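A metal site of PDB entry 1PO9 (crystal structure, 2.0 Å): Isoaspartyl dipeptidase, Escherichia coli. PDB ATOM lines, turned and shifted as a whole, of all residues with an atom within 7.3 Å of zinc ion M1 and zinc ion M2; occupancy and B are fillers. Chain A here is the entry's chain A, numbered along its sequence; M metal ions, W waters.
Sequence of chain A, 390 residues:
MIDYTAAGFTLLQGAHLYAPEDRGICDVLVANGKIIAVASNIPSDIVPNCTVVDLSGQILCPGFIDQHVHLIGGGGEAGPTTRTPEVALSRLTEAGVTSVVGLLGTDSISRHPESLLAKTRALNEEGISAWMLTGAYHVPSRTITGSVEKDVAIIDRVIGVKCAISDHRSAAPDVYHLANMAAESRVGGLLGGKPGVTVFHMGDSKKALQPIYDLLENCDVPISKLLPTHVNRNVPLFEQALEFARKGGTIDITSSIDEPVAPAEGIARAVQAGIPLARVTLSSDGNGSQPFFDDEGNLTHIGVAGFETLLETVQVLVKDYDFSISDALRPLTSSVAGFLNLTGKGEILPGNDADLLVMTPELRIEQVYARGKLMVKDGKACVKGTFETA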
ATOM      1  N   HIS A  68      19.263  -3.926 -15.618  1.00  0.00           N
ATOM      2  CA  HIS A  68      19.239  -2.892 -14.588  1.00  0.00           C
ATOM      3  C   HIS A  68      20.631  -2.301 -14.422  1.00  0.00           C
ATOM      4  O   HIS A  68      21.386  -2.684 -13.525  1.00  0.00           O
ATOM      5  CB  HIS A  68      18.763  -3.469 -13.256  1.00  0.00           C
ATOM      6  CG  HIS A  68      18.278  -2.442 -12.280  1.00  0.00           C
ATOM      7  ND1 HIS A  68      16.973  -2.374 -11.860  1.00  0.00           N
ATOM      8  CD2 HIS A  68      18.933  -1.431 -11.650  1.00  0.00           C
ATOM      9  CE1 HIS A  68      16.837  -1.372 -11.013  1.00  0.00           C
ATOM     10  NE2 HIS A  68      18.014  -0.779 -10.867  1.00  0.00           N
ATOM     11  N   VAL A  69      20.964  -1.353 -15.291  1.00  0.00           N
ATOM     12  CA  VAL A  69      22.270  -0.708 -15.270  1.00  0.00           C
ATOM     13  C   VAL A  69      22.155   0.795 -15.393  1.00  0.00           C
ATOM     14  O   VAL A  69      21.425   1.302 -16.247  1.00  0.00           O
ATOM     15  CB  VAL A  69      23.155  -1.233 -16.432  1.00  0.00           C
ATOM     16  CG1 VAL A  69      24.528  -0.558 -16.384  1.00  0.00           C
ATOM     17  CG2 VAL A  69      23.279  -2.745 -16.343  1.00  0.00           C
ATOM     18  N   HIS A  70      22.882   1.515 -14.547  1.00  0.00           N
ATOM     19  CA  HIS A  70      22.888   2.977 -14.582  1.00  0.00           C
ATOM     20  C   HIS A  70      23.980   3.368 -15.570  1.00  0.00           C
ATOM     21  O   HIS A  70      25.071   3.803 -15.202  1.00  0.00           O
ATOM     22  CB  HIS A  70      23.176   3.529 -13.190  1.00  0.00           C
ATOM     23  CG  HIS A  70      22.106   3.205 -12.200  1.00  0.00           C
ATOM     24  ND1 HIS A  70      21.018   4.019 -11.977  1.00  0.00           N
ATOM     25  CD2 HIS A  70      21.913   2.104 -11.431  1.00  0.00           C
ATOM     26  CE1 HIS A  70      20.201   3.441 -11.124  1.00  0.00           C
ATOM     27  NE2 HIS A  70      20.723   2.275 -10.770  1.00  0.00           N
ATOM     28  N   LEU A 103      18.863   2.688 -17.069  1.00  0.00           N
ATOM     29  CA  LEU A 103      17.797   3.344 -16.335  1.00  0.00           C
ATOM     30  C   LEU A 103      18.367   4.362 -15.367  1.00  0.00           C
ATOM     31  O   LEU A 103      19.580   4.406 -15.140  1.00  0.00           O
ATOM     32  CB  LEU A 103      16.968   2.290 -15.578  1.00  0.00           C
ATOM     33  CG  LEU A 103      17.746   1.172 -14.867  1.00  0.00           C
ATOM     34  CD1 LEU A 103      18.623   1.746 -13.766  1.00  0.00           C
ATOM     35  CD2 LEU A 103      16.751   0.177 -14.274  1.00  0.00           C
ATOM     36  N   LEU A 104      17.485   5.203 -14.824  1.00  0.00           N
ATOM     37  CA  LEU A 104      17.895   6.228 -13.866  1.00  0.00           C
ATOM     38  C   LEU A 104      17.418   5.792 -12.492  1.00  0.00           C
ATOM     39  O   LEU A 104      16.563   4.924 -12.362  1.00  0.00           O
ATOM     40  CB  LEU A 104      17.249   7.574 -14.206  1.00  0.00           C
ATOM     41  CG  LEU A 104      17.572   8.149 -15.581  1.00  0.00           C
ATOM     42  CD1 LEU A 104      16.904   9.518 -15.744  1.00  0.00           C
ATOM     43  CD2 LEU A 104      19.077   8.262 -15.740  1.00  0.00           C
ATOM     44  N   GLY A 105      17.972   6.427 -11.458  1.00  0.00           N
ATOM     45  CA  GLY A 105      17.597   6.063 -10.115  1.00  0.00           C
ATOM     46  C   GLY A 105      17.034   7.186  -9.269  1.00  0.00           C
ATOM     47  O   GLY A 105      16.119   7.914  -9.677  1.00  0.00           O
ATOM     48  N   THR A 106      17.582   7.312  -8.066  1.00  0.00           N
ATOM     49  CA  THR A 106      17.137   8.320  -7.129  1.00  0.00           C
ATOM     50  C   THR A 106      17.232   9.721  -7.720  1.00  0.00           C
ATOM     51  O   THR A 106      16.318  10.534  -7.581  1.00  0.00           O
ATOM     52  CB  THR A 106      17.983   8.290  -5.845  1.00  0.00           C
ATOM     53  OG1 THR A 106      17.989   6.956  -5.322  1.00  0.00           O
ATOM     54  CG2 THR A 106      17.418   9.236  -4.816  1.00  0.00           C
ATOM     55  N   TYR A 137      13.141   7.085 -10.232  1.00  0.00           N
ATOM     56  CA  TYR A 137      12.442   6.819  -8.981  1.00  0.00           C
ATOM     57  C   TYR A 137      11.196   7.697  -8.912  1.00  0.00           C
ATOM     58  O   TYR A 137      10.094   7.227  -8.595  1.00  0.00           O
ATOM     59  CB  TYR A 137      13.300   7.165  -7.758  1.00  0.00           C
ATOM     60  CG  TYR A 137      14.269   6.106  -7.279  1.00  0.00           C
ATOM     61  CD1 TYR A 137      14.716   6.119  -5.959  1.00  0.00           C
ATOM     62  CD2 TYR A 137      14.780   5.141  -8.145  1.00  0.00           C
ATOM     63  CE1 TYR A 137      15.665   5.200  -5.511  1.00  0.00           C
ATOM     64  CE2 TYR A 137      15.725   4.208  -7.698  1.00  0.00           C
ATOM     65  CZ  TYR A 137      16.162   4.255  -6.384  1.00  0.00           C
ATOM     66  OH  TYR A 137      17.120   3.363  -5.935  1.00  0.00           O
ATOM     67  N   KCX A 162      10.450   3.156 -15.353  1.00  0.00           N
ATOM     68  CA  KCX A 162      10.920   2.768 -14.034  1.00  0.00           C
ATOM     69  CB  KCX A 162      12.459   2.768 -14.017  1.00  0.00           C
ATOM     70  CG  KCX A 162      13.129   3.685 -12.986  1.00  0.00           C
ATOM     71  CD  KCX A 162      13.106   3.110 -11.579  1.00  0.00           C
ATOM     72  CE  KCX A 162      14.120   1.978 -11.356  1.00  0.00           C
ATOM     73  NZ  KCX A 162      15.478   2.442 -11.088  1.00  0.00           N
ATOM     74  C   KCX A 162      10.355   3.738 -13.014  1.00  0.00           C
ATOM     75  O   KCX A 162       9.954   4.849 -13.354  1.00  0.00           O
ATOM     76  CX  KCX A 162      16.249   1.941 -10.124  1.00  0.00           C
ATOM     77  OQ1 KCX A 162      15.834   1.023  -9.375  1.00  0.00           O
ATOM     78  OQ2 KCX A 162      17.420   2.363  -9.930  1.00  0.00           O
ATOM     79  N   CYS A 163      10.299   3.290 -11.769  1.00  0.00           N
ATOM     80  CA  CYS A 163       9.803   4.116 -10.671  1.00  0.00           C
ATOM     81  C   CYS A 163      10.286   3.451  -9.395  1.00  0.00           C
ATOM     82  O   CYS A 163      10.935   2.414  -9.434  1.00  0.00           O
ATOM     83  CB  CYS A 163       8.273   4.151 -10.680  1.00  0.00           C
ATOM     84  SG  CYS A 163       7.514   2.572 -10.199  1.00  0.00           S
ATOM     85  N   ALA A 164       9.973   4.062  -8.258  1.00  0.00           N
ATOM     86  CA  ALA A 164      10.360   3.531  -6.964  1.00  0.00           C
ATOM     87  C   ALA A 164       9.156   3.541  -6.035  1.00  0.00           C
ATOM     88  O   ALA A 164       8.373   4.503  -6.035  1.00  0.00           O
ATOM     89  CB  ALA A 164      11.487   4.354  -6.366  1.00  0.00           C
ATOM     90  N   ASP A 167      10.001   2.859  -0.636  1.00  0.00           N
ATOM     91  CA  ASP A 167      11.401   3.237  -0.408  1.00  0.00           C
ATOM     92  C   ASP A 167      11.468   4.668   0.109  1.00  0.00           C
ATOM     93  O   ASP A 167      10.739   5.547  -0.367  1.00  0.00           O
ATOM     94  CB  ASP A 167      12.177   3.124  -1.726  1.00  0.00           C
ATOM     95  CG  ASP A 167      13.668   3.385  -1.549  1.00  0.00           C
ATOM     96  OD1 ASP A 167      14.428   2.409  -1.376  1.00  0.00           O
ATOM     97  OD2 ASP A 167      14.085   4.561  -1.599  1.00  0.00           O
ATOM     98  N   ARG A 169      13.197   6.969  -0.550  1.00  0.00           N
ATOM     99  CA  ARG A 169      13.610   7.941  -1.558  1.00  0.00           C
ATOM    100  C   ARG A 169      12.563   8.022  -2.666  1.00  0.00           C
ATOM    101  O   ARG A 169      12.843   8.541  -3.752  1.00  0.00           O
ATOM    102  CB  ARG A 169      14.928   7.535  -2.205  1.00  0.00           C
ATOM    103  CG  ARG A 169      16.019   7.126  -1.246  1.00  0.00           C
ATOM    104  CD  ARG A 169      16.963   6.234  -2.011  1.00  0.00           C
ATOM    105  NE  ARG A 169      17.831   5.453  -1.145  1.00  0.00           N
ATOM    106  CZ  ARG A 169      18.445   4.343  -1.526  1.00  0.00           C
ATOM    107  NH1 ARG A 169      18.281   3.895  -2.765  1.00  0.00           N
ATOM    108  NH2 ARG A 169      19.226   3.687  -0.675  1.00  0.00           N
ATOM    109  N   PHE A 200       9.744  -1.686 -10.894  1.00  0.00           N
ATOM    110  CA  PHE A 200       9.600  -1.053  -9.591  1.00  0.00           C
ATOM    111  C   PHE A 200      10.800  -1.237  -8.664  1.00  0.00           C
ATOM    112  O   PHE A 200      11.068  -2.355  -8.204  1.00  0.00           O
ATOM    113  CB  PHE A 200       8.367  -1.606  -8.855  1.00  0.00           C
ATOM    114  CG  PHE A 200       7.088  -1.441  -9.605  1.00  0.00           C
ATOM    115  CD1 PHE A 200       6.765  -2.297 -10.651  1.00  0.00           C
ATOM    116  CD2 PHE A 200       6.190  -0.439  -9.243  1.00  0.00           C
ATOM    117  CE1 PHE A 200       5.553  -2.163 -11.339  1.00  0.00           C
ATOM    118  CE2 PHE A 200       4.973  -0.304  -9.917  1.00  0.00           C
ATOM    119  CZ  PHE A 200       4.660  -1.163 -10.960  1.00  0.00           C
ATOM    120  N   HIS A 201      11.515  -0.152  -8.385  1.00  0.00           N
ATOM    121  CA  HIS A 201      12.642  -0.223  -7.462  1.00  0.00           C
ATOM    122  C   HIS A 201      11.965  -0.417  -6.112  1.00  0.00           C
ATOM    123  O   HIS A 201      11.168   0.409  -5.696  1.00  0.00           O
ATOM    124  CB  HIS A 201      13.420   1.094  -7.425  1.00  0.00           C
ATOM    125  CG  HIS A 201      14.281   1.246  -6.202  1.00  0.00           C
ATOM    126  ND1 HIS A 201      15.537   0.687  -6.096  1.00  0.00           N
ATOM    127  CD2 HIS A 201      14.035   1.826  -5.003  1.00  0.00           C
ATOM    128  CE1 HIS A 201      16.029   0.920  -4.889  1.00  0.00           C
ATOM    129  NE2 HIS A 201      15.137   1.612  -4.205  1.00  0.00           N
ATOM    130  N   MET A 202      12.286  -1.522  -5.448  1.00  0.00           N
ATOM    131  CA  MET A 202      11.695  -1.802  -4.138  1.00  0.00           C
ATOM    132  C   MET A 202      12.614  -1.323  -3.024  1.00  0.00           C
ATOM    133  O   MET A 202      13.831  -1.433  -3.113  1.00  0.00           O
ATOM    134  CB  MET A 202      11.466  -3.302  -3.950  1.00  0.00           C
ATOM    135  CG  MET A 202      10.532  -3.957  -4.967  1.00  0.00           C
ATOM    136  SD  MET A 202       8.981  -3.083  -5.230  1.00  0.00           S
ATOM    137  CE  MET A 202       8.311  -3.105  -3.554  1.00  0.00           C
ATOM    138  N   THR A 229      11.954  -5.128  -8.525  1.00  0.00           N
ATOM    139  CA  THR A 229      13.377  -5.463  -8.522  1.00  0.00           C
ATOM    140  C   THR A 229      13.991  -5.230  -7.156  1.00  0.00           C
ATOM    141  O   THR A 229      13.386  -4.591  -6.297  1.00  0.00           O
ATOM    142  CB  THR A 229      14.136  -4.687  -9.625  1.00  0.00           C
ATOM    143  OG1 THR A 229      15.502  -5.143  -9.670  1.00  0.00           O
ATOM    144  CG2 THR A 229      14.117  -3.197  -9.373  1.00  0.00           C
ATOM    145  N   HIS A 230      15.193  -5.761  -6.935  1.00  0.00           N
ATOM    146  CA  HIS A 230      15.862  -5.647  -5.646  1.00  0.00           C
ATOM    147  C   HIS A 230      15.031  -6.412  -4.613  1.00  0.00           C
ATOM    148  O   HIS A 230      15.093  -6.123  -3.425  1.00  0.00           O
ATOM    149  CB  HIS A 230      15.978  -4.184  -5.205  1.00  0.00           C
ATOM    150  CG  HIS A 230      16.678  -3.296  -6.194  1.00  0.00           C
ATOM    151  ND1 HIS A 230      17.919  -3.593  -6.709  1.00  0.00           N
ATOM    152  CD2 HIS A 230      16.298  -2.124  -6.755  1.00  0.00           C
ATOM    153  CE1 HIS A 230      18.279  -2.639  -7.554  1.00  0.00           C
ATOM    154  NE2 HIS A 230      17.314  -1.744  -7.603  1.00  0.00           N
ATOM    155  N   ARG A 233      16.476  -7.567  -1.183  1.00  0.00           N
ATOM    156  CA  ARG A 233      17.002  -6.587  -0.220  1.00  0.00           C
ATOM    157  C   ARG A 233      16.581  -6.844   1.226  1.00  0.00           C
ATOM    158  O   ARG A 233      17.271  -6.412   2.156  1.00  0.00           O
ATOM    159  CB  ARG A 233      16.610  -5.172  -0.616  1.00  0.00           C
ATOM    160  CG  ARG A 233      15.118  -4.934  -0.605  1.00  0.00           C
ATOM    161  CD  ARG A 233      14.793  -3.446  -0.499  1.00  0.00           C
ATOM    162  NE  ARG A 233      15.445  -2.654  -1.534  1.00  0.00           N
ATOM    163  CZ  ARG A 233      16.491  -1.858  -1.326  1.00  0.00           C
ATOM    164  NH1 ARG A 233      17.003  -1.728  -0.113  1.00  0.00           N
ATOM    165  NH2 ARG A 233      17.015  -1.181  -2.329  1.00  0.00           N
ATOM    166  N   THR A 254      18.588  -8.834  -7.523  1.00  0.00           N
ATOM    167  CA  THR A 254      19.783  -8.040  -7.803  1.00  0.00           C
ATOM    168  C   THR A 254      21.051  -8.756  -7.346  1.00  0.00           C
ATOM    169  O   THR A 254      21.181  -9.134  -6.186  1.00  0.00           O
ATOM    170  CB  THR A 254      19.704  -6.656  -7.137  1.00  0.00           C
ATOM    171  OG1 THR A 254      18.504  -6.000  -7.560  1.00  0.00           O
ATOM    172  CG2 THR A 254      20.903  -5.821  -7.546  1.00  0.00           C
ATOM    173  N   SER A 284      22.283  -6.521 -12.362  1.00  0.00           N
ATOM    174  CA  SER A 284      23.385  -6.076 -11.514  1.00  0.00           C
ATOM    175  C   SER A 284      23.235  -4.754 -10.769  1.00  0.00           C
ATOM    176  O   SER A 284      23.844  -4.568  -9.715  1.00  0.00           O
ATOM    177  CB  SER A 284      24.660  -5.986 -12.359  1.00  0.00           C
ATOM    178  OG  SER A 284      24.544  -4.951 -13.323  1.00  0.00           O
ATOM    179  N   ASP A 285      22.443  -3.852 -11.328  1.00  0.00           N
ATOM    180  CA  ASP A 285      22.283  -2.521 -10.767  1.00  0.00           C
ATOM    181  C   ASP A 285      23.675  -1.922 -10.842  1.00  0.00           C
ATOM    182  O   ASP A 285      24.124  -1.197  -9.961  1.00  0.00           O
ATOM    183  CB  ASP A 285      21.801  -2.580  -9.310  1.00  0.00           C
ATOM    184  CG  ASP A 285      21.315  -1.232  -8.814  1.00  0.00           C
ATOM    185  OD1 ASP A 285      20.951  -0.382  -9.660  1.00  0.00           O
ATOM    186  OD2 ASP A 285      21.280  -1.018  -7.579  1.00  0.00           O
ATOM    187  N   GLY A 286      24.360  -2.267 -11.934  1.00  0.00           N
ATOM    188  CA  GLY A 286      25.713  -1.814 -12.160  1.00  0.00           C
ATOM    189  C   GLY A 286      25.857  -0.306 -12.227  1.00  0.00           C
ATOM    190  O   GLY A 286      24.996   0.389 -12.787  1.00  0.00           O
ATOM    191  N   GLY A 288      25.533   1.704  -9.978  1.00  0.00           N
ATOM    192  CA  GLY A 288      24.578   2.379  -9.103  1.00  0.00           C
ATOM    193  C   GLY A 288      25.192   2.672  -7.741  1.00  0.00           C
ATOM    194  O   GLY A 288      26.416   2.753  -7.609  1.00  0.00           O
HETATM  195 ZN    ZN M   1      16.853   0.532  -7.538  1.00  0.00          ZN
HETATM  196 ZN    ZN M   2      19.120   0.995  -9.858  1.00  0.00          ZN
HETATM  197  O   HOH W   1      18.842   0.882  -7.867  1.00  0.00           O
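OH of Tyr 137 lies close to NE2 of His 201, at 3.2 Å. NE2 of His 201 lies within hydrogen-bond range of OD1 of Asp 167 (3.0 Å). NZ of KCX 162 sits at hydrogen-bond distance from the backbone carbonyl oxygen (O) of Leu 104, 3.0 Å away. O of Gly 286 is in hydrogen-bond range of N of His 70. The side-chain hydroxyl (OG1) of Thr 254 sits at hydrogen-bond distance from a ring nitrogen (ND1) of His 230, at 2.6 Å. The backbone NH of Tyr 137 sits at hydrogen-bond distance from the backbone carbonyl oxygen of Gly 105 (3.1 Å). NH1 of Arg 169 is in hydrogen-bond range of OH of Tyr 137 (3.4 Å). The backbone NH (N) of Ala 164 sits at hydrogen-bond distance from the backbone carbonyl oxygen (O) of Tyr 137 (3.2 Å).
Tyr 137 touches zinc ion M1 (OH to ZN, 3.3 Å). Of the 24 residues printed, 5 come within 4 Å of zinc ion M1. Along chain A the residues within 4 Å of zinc ion M1 span positions 68 to 230.
Five residues have an atom within 4 Å of zinc ion M2: His 68, His 70, KCX 162, His 230 and Asp 285.
Zinc ion M1 is bound by a ring nitrogen (ND1) of His 201 (2.0 Å), water W1 (2.0 Å), OQ1 of KCX 162 (2.2 Å) and a ring nitrogen (NE2) of His 230 (2.3 Å). Zinc ion M1 has four donor atoms within binding distance.
Zinc ion M2 is bound by water W1 (2.0 Å), OQ2 of KCX 162 (2.2 Å), a ring nitrogen (NE2) of His 70 (2.2 Å), the side-chain carboxylate (OD1) of Asp 285 (2.3 Å) and a ring nitrogen (NE2) of His 68 (2.3 Å).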
